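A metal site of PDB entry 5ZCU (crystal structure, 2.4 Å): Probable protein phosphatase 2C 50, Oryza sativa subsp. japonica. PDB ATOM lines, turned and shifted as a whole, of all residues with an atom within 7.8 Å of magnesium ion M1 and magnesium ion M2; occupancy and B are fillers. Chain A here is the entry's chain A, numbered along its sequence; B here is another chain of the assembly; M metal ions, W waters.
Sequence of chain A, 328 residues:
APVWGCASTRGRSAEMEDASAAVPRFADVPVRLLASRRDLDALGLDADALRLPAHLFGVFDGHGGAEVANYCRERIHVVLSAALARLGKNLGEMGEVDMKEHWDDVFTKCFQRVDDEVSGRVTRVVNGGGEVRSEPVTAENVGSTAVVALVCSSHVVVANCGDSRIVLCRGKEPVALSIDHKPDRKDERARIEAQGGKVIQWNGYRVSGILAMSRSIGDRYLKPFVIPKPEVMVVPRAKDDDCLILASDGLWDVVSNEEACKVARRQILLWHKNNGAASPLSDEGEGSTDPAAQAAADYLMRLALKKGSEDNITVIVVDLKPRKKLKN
Magnesium ion M2 is bound by O of Gly 62 (2.1 Å), water W3 (2.1 Å), water W2 (2.2 Å), water W5 (2.3 Å) and OD1 of Asp 61 (2.3 Å). Magnesium ion M2 has five donor atoms within binding distance.
Merely in contact with magnesium ion M2: Glu 17. The nearest printed residue that does not touch magnesium ion M2 is His 63 (4.2 Å).
Water W2 lies within hydrogen-bond range of the side-chain carboxylate of Asp 18 (2.8 Å) and the side-chain amide oxygen of Asn 312 (2.9 Å).
The backbone NH (N) of Glu 17 lies within hydrogen-bond range of the side-chain amide oxygen (OD1) of Asn 312. The backbone carbonyl oxygen (O) of Asp 61 lies within hydrogen-bond range of the backbone NH (N) of Thr 145 (2.8 Å). O of Asp 61 lies close to OG of Ser 144 (3.4 Å). The side-chain carboxylate (OE2) of Glu 17 is in hydrogen-bond range of the backbone NH (N) of Gly 65 (2.9 Å). The side-chain hydroxyl (OG) of Ser 71 of chain B lies close to the side-chain carboxylate (OE2) of Glu 17 (3.4 Å). O of Glu 17 lies within hydrogen-bond range of N of Gly 62 (2.9 Å).
Within 4 Å of magnesium ion M1: Asp 61, Asp 249 and Asp 311.
Magnesium ion M1 is bound by the side-chain carboxylate of Asp 61 (1.9 Å), the side-chain carboxylate of Asp 311 (2.0 Å), water W1 (2.0 Å), the side-chain carboxylate of Asp 249 (2.1 Å), water W3 (2.2 Å) and water W4 (2.3 Å). Magnesium ion M1 has six donor atoms within binding distance.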
ATOM      1  N   SER A  13      21.041  18.968  23.973  1.00  0.00           N
ATOM      2  CA  SER A  13      21.336  18.665  22.590  1.00  0.00           C
ATOM      3  C   SER A  13      20.359  19.393  21.674  1.00  0.00           C
ATOM      4  O   SER A  13      19.215  19.679  22.036  1.00  0.00           O
ATOM      5  CB  SER A  13      21.272  17.160  22.356  1.00  0.00           C
ATOM      6  OG  SER A  13      22.427  16.500  22.846  1.00  0.00           O
ATOM      7  N   GLU A  15      18.998  18.449  18.644  1.00  0.00           N
ATOM      8  CA  GLU A  15      17.934  17.623  18.103  1.00  0.00           C
ATOM      9  C   GLU A  15      17.815  16.332  18.889  1.00  0.00           C
ATOM     10  O   GLU A  15      18.769  15.875  19.532  1.00  0.00           O
ATOM     11  CB  GLU A  15      18.185  17.319  16.618  1.00  0.00           C
ATOM     12  CG  GLU A  15      18.750  18.510  15.845  1.00  0.00           C
ATOM     13  CD  GLU A  15      19.650  18.104  14.705  1.00  0.00           C
ATOM     14  OE1 GLU A  15      20.729  18.717  14.549  1.00  0.00           O
ATOM     15  OE2 GLU A  15      19.285  17.178  13.960  1.00  0.00           O
ATOM     16  N   MET A  16      16.621  15.743  18.849  1.00  0.00           N
ATOM     17  CA  MET A  16      16.326  14.499  19.549  1.00  0.00           C
ATOM     18  C   MET A  16      16.555  13.340  18.578  1.00  0.00           C
ATOM     19  O   MET A  16      15.835  13.215  17.585  1.00  0.00           O
ATOM     20  CB  MET A  16      14.897  14.504  20.075  1.00  0.00           C
ATOM     21  CG  MET A  16      14.511  13.272  20.866  1.00  0.00           C
ATOM     22  SD  MET A  16      15.740  12.830  22.103  1.00  0.00           S
ATOM     23  CE  MET A  16      14.790  11.721  23.148  1.00  0.00           C
ATOM     24  N   GLU A  17      17.543  12.502  18.882  1.00  0.00           N
ATOM     25  CA  GLU A  17      17.843  11.332  18.058  1.00  0.00           C
ATOM     26  C   GLU A  17      17.761  10.035  18.841  1.00  0.00           C
ATOM     27  O   GLU A  17      18.102   8.974  18.301  1.00  0.00           O
ATOM     28  CB  GLU A  17      19.217  11.498  17.397  1.00  0.00           C
ATOM     29  CG  GLU A  17      19.300  12.724  16.504  1.00  0.00           C
ATOM     30  CD  GLU A  17      20.680  12.969  15.949  1.00  0.00           C
ATOM     31  OE1 GLU A  17      21.665  12.544  16.596  1.00  0.00           O
ATOM     32  OE2 GLU A  17      20.791  13.589  14.875  1.00  0.00           O
ATOM     33  N   ASP A  18      17.325  10.083  20.092  1.00  0.00           N
ATOM     34  CA  ASP A  18      17.055   8.886  20.873  1.00  0.00           C
ATOM     35  C   ASP A  18      15.650   8.387  20.578  1.00  0.00           C
ATOM     36  O   ASP A  18      14.752   9.164  20.246  1.00  0.00           O
ATOM     37  CB  ASP A  18      17.216   9.159  22.364  1.00  0.00           C
ATOM     38  CG  ASP A  18      18.630   8.926  22.855  1.00  0.00           C
ATOM     39  OD1 ASP A  18      19.520   8.671  22.025  1.00  0.00           O
ATOM     40  OD2 ASP A  18      18.846   9.008  24.089  1.00  0.00           O
ATOM     41  N   PHE A  60      17.298   3.047  21.692  1.00  0.00           N
ATOM     42  CA  PHE A  60      18.019   3.191  20.433  1.00  0.00           C
ATOM     43  C   PHE A  60      18.591   4.594  20.337  1.00  0.00           C
ATOM     44  O   PHE A  60      17.876   5.553  20.031  1.00  0.00           O
ATOM     45  CB  PHE A  60      17.096   2.878  19.259  1.00  0.00           C
ATOM     46  CG  PHE A  60      16.229   1.661  19.484  1.00  0.00           C
ATOM     47  CD1 PHE A  60      16.746   0.385  19.309  1.00  0.00           C
ATOM     48  CD2 PHE A  60      14.919   1.790  19.897  1.00  0.00           C
ATOM     49  CE1 PHE A  60      15.966  -0.726  19.525  1.00  0.00           C
ATOM     50  CE2 PHE A  60      14.131   0.685  20.115  1.00  0.00           C
ATOM     51  CZ  PHE A  60      14.650  -0.584  19.927  1.00  0.00           C
ATOM     52  N   ASP A  61      19.892   4.718  20.601  1.00  0.00           N
ATOM     53  CA  ASP A  61      20.610   5.991  20.518  1.00  0.00           C
ATOM     54  C   ASP A  61      21.033   6.204  19.068  1.00  0.00           C
ATOM     55  O   ASP A  61      21.966   5.559  18.587  1.00  0.00           O
ATOM     56  CB  ASP A  61      21.811   5.983  21.460  1.00  0.00           C
ATOM     57  CG  ASP A  61      22.495   7.347  21.553  1.00  0.00           C
ATOM     58  OD1 ASP A  61      22.344   8.180  20.633  1.00  0.00           O
ATOM     59  OD2 ASP A  61      23.202   7.573  22.557  1.00  0.00           O
ATOM     60  N   GLY A  62      20.350   7.111  18.384  1.00  0.00           N
ATOM     61  CA  GLY A  62      20.706   7.407  17.015  1.00  0.00           C
ATOM     62  C   GLY A  62      21.838   8.415  16.896  1.00  0.00           C
ATOM     63  O   GLY A  62      22.074   9.222  17.802  1.00  0.00           O
ATOM     64  N   HIS A  63      22.539   8.353  15.777  1.00  0.00           N
ATOM     65  CA  HIS A  63      23.572   9.333  15.441  1.00  0.00           C
ATOM     66  C   HIS A  63      23.468   9.658  13.955  1.00  0.00           C
ATOM     67  O   HIS A  63      23.002   8.847  13.158  1.00  0.00           O
ATOM     68  CB  HIS A  63      24.981   8.831  15.779  1.00  0.00           C
ATOM     69  CG  HIS A  63      25.237   7.414  15.362  1.00  0.00           C
ATOM     70  ND1 HIS A  63      25.037   6.344  16.204  1.00  0.00           N
ATOM     71  CD2 HIS A  63      25.691   6.892  14.198  1.00  0.00           C
ATOM     72  CE1 HIS A  63      25.347   5.228  15.587  1.00  0.00           C
ATOM     73  NE2 HIS A  63      25.748   5.531  14.362  1.00  0.00           N
ATOM     74  N   GLY A  64      23.899  10.870  13.608  1.00  0.00           N
ATOM     75  CA  GLY A  64      23.763  11.359  12.252  1.00  0.00           C
ATOM     76  C   GLY A  64      22.335  11.696  11.861  1.00  0.00           C
ATOM     77  O   GLY A  64      22.082  11.969  10.687  1.00  0.00           O
ATOM     78  N   GLY A  65      21.405  11.660  12.796  1.00  0.00           N
ATOM     79  CA  GLY A  65      20.005  11.811  12.444  1.00  0.00           C
ATOM     80  C   GLY A  65      19.176  10.871  13.278  1.00  0.00           C
ATOM     81  O   GLY A  65      19.742  10.062  14.019  1.00  0.00           O
ATOM     82  N   ALA A  69      17.188   5.276  14.323  1.00  0.00           N
ATOM     83  CA  ALA A  69      16.695   4.893  15.653  1.00  0.00           C
ATOM     84  C   ALA A  69      15.185   4.700  15.652  1.00  0.00           C
ATOM     85  O   ALA A  69      14.669   3.764  16.267  1.00  0.00           O
ATOM     86  CB  ALA A  69      17.105   5.930  16.691  1.00  0.00           C
ATOM     87  N   GLY A 143      23.020   6.190  11.806  1.00  0.00           N
ATOM     88  CA  GLY A 143      23.004   4.906  12.471  1.00  0.00           C
ATOM     89  C   GLY A 143      22.352   5.023  13.835  1.00  0.00           C
ATOM     90  O   GLY A 143      21.864   6.091  14.228  1.00  0.00           O
ATOM     91  N   SER A 144      22.352   3.912  14.566  1.00  0.00           N
ATOM     92  CA  SER A 144      21.738   3.876  15.884  1.00  0.00           C
ATOM     93  C   SER A 144      22.266   2.691  16.676  1.00  0.00           C
ATOM     94  O   SER A 144      22.531   1.634  16.102  1.00  0.00           O
ATOM     95  CB  SER A 144      20.207   3.791  15.787  1.00  0.00           C
ATOM     96  OG  SER A 144      19.629   3.639  17.074  1.00  0.00           O
ATOM     97  N   THR A 145      22.426   2.884  17.983  1.00  0.00           N
ATOM     98  CA  THR A 145      22.611   1.757  18.878  1.00  0.00           C
ATOM     99  C   THR A 145      21.298   1.000  19.056  1.00  0.00           C
ATOM    100  O   THR A 145      20.217   1.481  18.693  1.00  0.00           O
ATOM    101  CB  THR A 145      23.115   2.227  20.249  1.00  0.00           C
ATOM    102  OG1 THR A 145      21.998   2.571  21.073  1.00  0.00           O
ATOM    103  CG2 THR A 145      23.996   3.453  20.093  1.00  0.00           C
ATOM    104  N   ASP A 163      26.804   1.322  22.251  1.00  0.00           N
ATOM    105  CA  ASP A 163      27.238   1.848  23.532  1.00  0.00           C
ATOM    106  C   ASP A 163      26.073   2.269  24.431  1.00  0.00           C
ATOM    107  O   ASP A 163      26.296   2.984  25.411  1.00  0.00           O
ATOM    108  CB  ASP A 163      28.206   3.018  23.327  1.00  0.00           C
ATOM    109  CG  ASP A 163      27.516   4.294  22.862  1.00  0.00           C
ATOM    110  OD1 ASP A 163      26.400   4.212  22.294  1.00  0.00           O
ATOM    111  OD2 ASP A 163      28.104   5.375  23.040  1.00  0.00           O
ATOM    112  N   SER A 164      24.855   1.851  24.111  1.00  0.00           N
ATOM    113  CA  SER A 164      23.801   1.907  25.107  1.00  0.00           C
ATOM    114  C   SER A 164      23.978   0.747  26.088  1.00  0.00           C
ATOM    115  O   SER A 164      24.730  -0.196  25.850  1.00  0.00           O
ATOM    116  CB  SER A 164      22.425   1.849  24.436  1.00  0.00           C
ATOM    117  OG  SER A 164      22.125   3.069  23.783  1.00  0.00           O
ATOM    118  N   MET A 213      31.764   3.765  18.277  1.00  0.00           N
ATOM    119  CA  MET A 213      31.220   2.438  18.514  1.00  0.00           C
ATOM    120  C   MET A 213      31.697   1.497  17.415  1.00  0.00           C
ATOM    121  O   MET A 213      31.936   1.913  16.285  1.00  0.00           O
ATOM    122  CB  MET A 213      29.681   2.430  18.529  1.00  0.00           C
ATOM    123  CG  MET A 213      29.023   3.631  19.181  1.00  0.00           C
ATOM    124  SD  MET A 213      27.462   4.059  18.393  1.00  0.00           S
ATOM    125  CE  MET A 213      26.714   2.446  18.223  1.00  0.00           C
ATOM    126  N   SER A 248      20.195   5.091  27.214  1.00  0.00           N
ATOM    127  CA  SER A 248      21.240   5.554  26.318  1.00  0.00           C
ATOM    128  C   SER A 248      22.423   6.087  27.139  1.00  0.00           C
ATOM    129  O   SER A 248      22.316   6.311  28.345  1.00  0.00           O
ATOM    130  CB  SER A 248      20.703   6.626  25.371  1.00  0.00           C
ATOM    131  OG  SER A 248      20.142   7.701  26.100  1.00  0.00           O
ATOM    132  N   ASP A 249      23.541   6.317  26.456  1.00  0.00           N
ATOM    133  CA  ASP A 249      24.732   6.806  27.149  1.00  0.00           C
ATOM    134  C   ASP A 249      24.546   8.211  27.713  1.00  0.00           C
ATOM    135  O   ASP A 249      25.423   8.674  28.444  1.00  0.00           O
ATOM    136  CB  ASP A 249      25.946   6.764  26.226  1.00  0.00           C
ATOM    137  CG  ASP A 249      25.802   7.670  25.018  1.00  0.00           C
ATOM    138  OD1 ASP A 249      24.722   8.251  24.826  1.00  0.00           O
ATOM    139  OD2 ASP A 249      26.791   7.803  24.262  1.00  0.00           O
ATOM    140  N   GLY A 250      23.445   8.890  27.405  1.00  0.00           N
ATOM    141  CA  GLY A 250      23.171  10.163  28.059  1.00  0.00           C
ATOM    142  C   GLY A 250      23.070  10.047  29.567  1.00  0.00           C
ATOM    143  O   GLY A 250      23.433  10.977  30.290  1.00  0.00           O
ATOM    144  N   LEU A 251      22.625   8.895  30.064  1.00  0.00           N
ATOM    145  CA  LEU A 251      22.589   8.646  31.499  1.00  0.00           C
ATOM    146  C   LEU A 251      23.915   8.077  31.980  1.00  0.00           C
ATOM    147  O   LEU A 251      24.495   8.575  32.953  1.00  0.00           O
ATOM    148  CB  LEU A 251      21.442   7.702  31.855  1.00  0.00           C
ATOM    149  CG  LEU A 251      21.436   7.229  33.312  1.00  0.00           C
ATOM    150  CD1 LEU A 251      20.547   8.123  34.164  1.00  0.00           C
ATOM    151  CD2 LEU A 251      21.017   5.770  33.440  1.00  0.00           C
ATOM    152  N   ASP A 253      26.821   8.314  30.946  1.00  0.00           N
ATOM    153  CA  ASP A 253      27.980   9.187  30.882  1.00  0.00           C
ATOM    154  C   ASP A 253      28.218   9.923  32.203  1.00  0.00           C
ATOM    155  O   ASP A 253      29.356  10.276  32.512  1.00  0.00           O
ATOM    156  CB  ASP A 253      27.813  10.208  29.753  1.00  0.00           C
ATOM    157  CG  ASP A 253      28.176   9.648  28.392  1.00  0.00           C
ATOM    158  OD1 ASP A 253      28.746   8.541  28.333  1.00  0.00           O
ATOM    159  OD2 ASP A 253      27.896  10.317  27.376  1.00  0.00           O
ATOM    160  N   ASP A 311      23.889  15.114  26.324  1.00  0.00           N
ATOM    161  CA  ASP A 311      23.346  14.261  25.292  1.00  0.00           C
ATOM    162  C   ASP A 311      21.826  14.106  25.432  1.00  0.00           C
ATOM    163  O   ASP A 311      21.222  14.538  26.421  1.00  0.00           O
ATOM    164  CB  ASP A 311      24.022  12.882  25.340  1.00  0.00           C
ATOM    165  CG  ASP A 311      23.811  12.089  24.060  1.00  0.00           C
ATOM    166  OD1 ASP A 311      23.223  12.628  23.107  1.00  0.00           O
ATOM    167  OD2 ASP A 311      24.240  10.917  24.026  1.00  0.00           O
ATOM    168  N   ASN A 312      21.213  13.513  24.412  1.00  0.00           N
ATOM    169  CA  ASN A 312      19.863  12.987  24.570  1.00  0.00           C
ATOM    170  C   ASN A 312      19.836  11.981  25.712  1.00  0.00           C
ATOM    171  O   ASN A 312      20.801  11.246  25.933  1.00  0.00           O
ATOM    172  CB  ASN A 312      19.402  12.307  23.269  1.00  0.00           C
ATOM    173  CG  ASN A 312      19.269  13.285  22.111  1.00  0.00           C
ATOM    174  OD1 ASN A 312      19.196  12.879  20.943  1.00  0.00           O
ATOM    175  ND2 ASN A 312      19.215  14.575  22.417  1.00  0.00           N
ATOM    176  N   ILE A 313      18.724  11.950  26.439  1.00  0.00           N
ATOM    177  CA  ILE A 313      18.548  11.045  27.563  1.00  0.00           C
ATOM    178  C   ILE A 313      17.320  10.191  27.303  1.00  0.00           C
ATOM    179  O   ILE A 313      16.271  10.713  26.909  1.00  0.00           O
ATOM    180  CB  ILE A 313      18.407  11.797  28.899  1.00  0.00           C
ATOM    181  CG1 ILE A 313      19.413  12.964  29.051  1.00  0.00           C
ATOM    182  CG2 ILE A 313      18.565  10.858  30.063  1.00  0.00           C
ATOM    183  CD1 ILE A 313      20.805  12.574  29.444  1.00  0.00           C
ATOM    184  N   SER B  71      25.685  14.633  14.762  1.00  0.00           N
ATOM    185  CA  SER B  71      26.133  13.745  15.817  1.00  0.00           C
ATOM    186  C   SER B  71      26.925  12.572  15.247  1.00  0.00           C
ATOM    187  O   SER B  71      26.911  12.295  14.045  1.00  0.00           O
ATOM    188  CB  SER B  71      24.938  13.239  16.630  1.00  0.00           C
ATOM    189  OG  SER B  71      23.910  12.758  15.779  1.00  0.00           O
ATOM    190  N   GLY B  72      27.626  11.876  16.132  1.00  0.00           N
ATOM    191  CA  GLY B  72      28.392  10.714  15.736  1.00  0.00           C
ATOM    192  C   GLY B  72      29.752  11.022  15.136  1.00  0.00           C
ATOM    193  O   GLY B  72      30.289  10.188  14.401  1.00  0.00           O
HETATM  194 MG    MG M   1      23.989   9.202  23.070  1.00  0.00          MG
HETATM  195 MG    MG M   2      22.685  10.205  19.508  1.00  0.00          MG
HETATM  196  O   HOH W   1      25.784   9.233  22.088  1.00  0.00           O
HETATM  197  O   HOH W   2      20.700  10.495  20.313  1.00  0.00           O
HETATM  198  O   HOH W   3      23.181  10.541  21.484  1.00  0.00           O
HETATM  199  O   HOH W   4      21.788   9.675  23.686  1.00  0.00           O
HETATM  200  O   HOH W   5      24.738   9.114  19.248  1.00  0.00           O
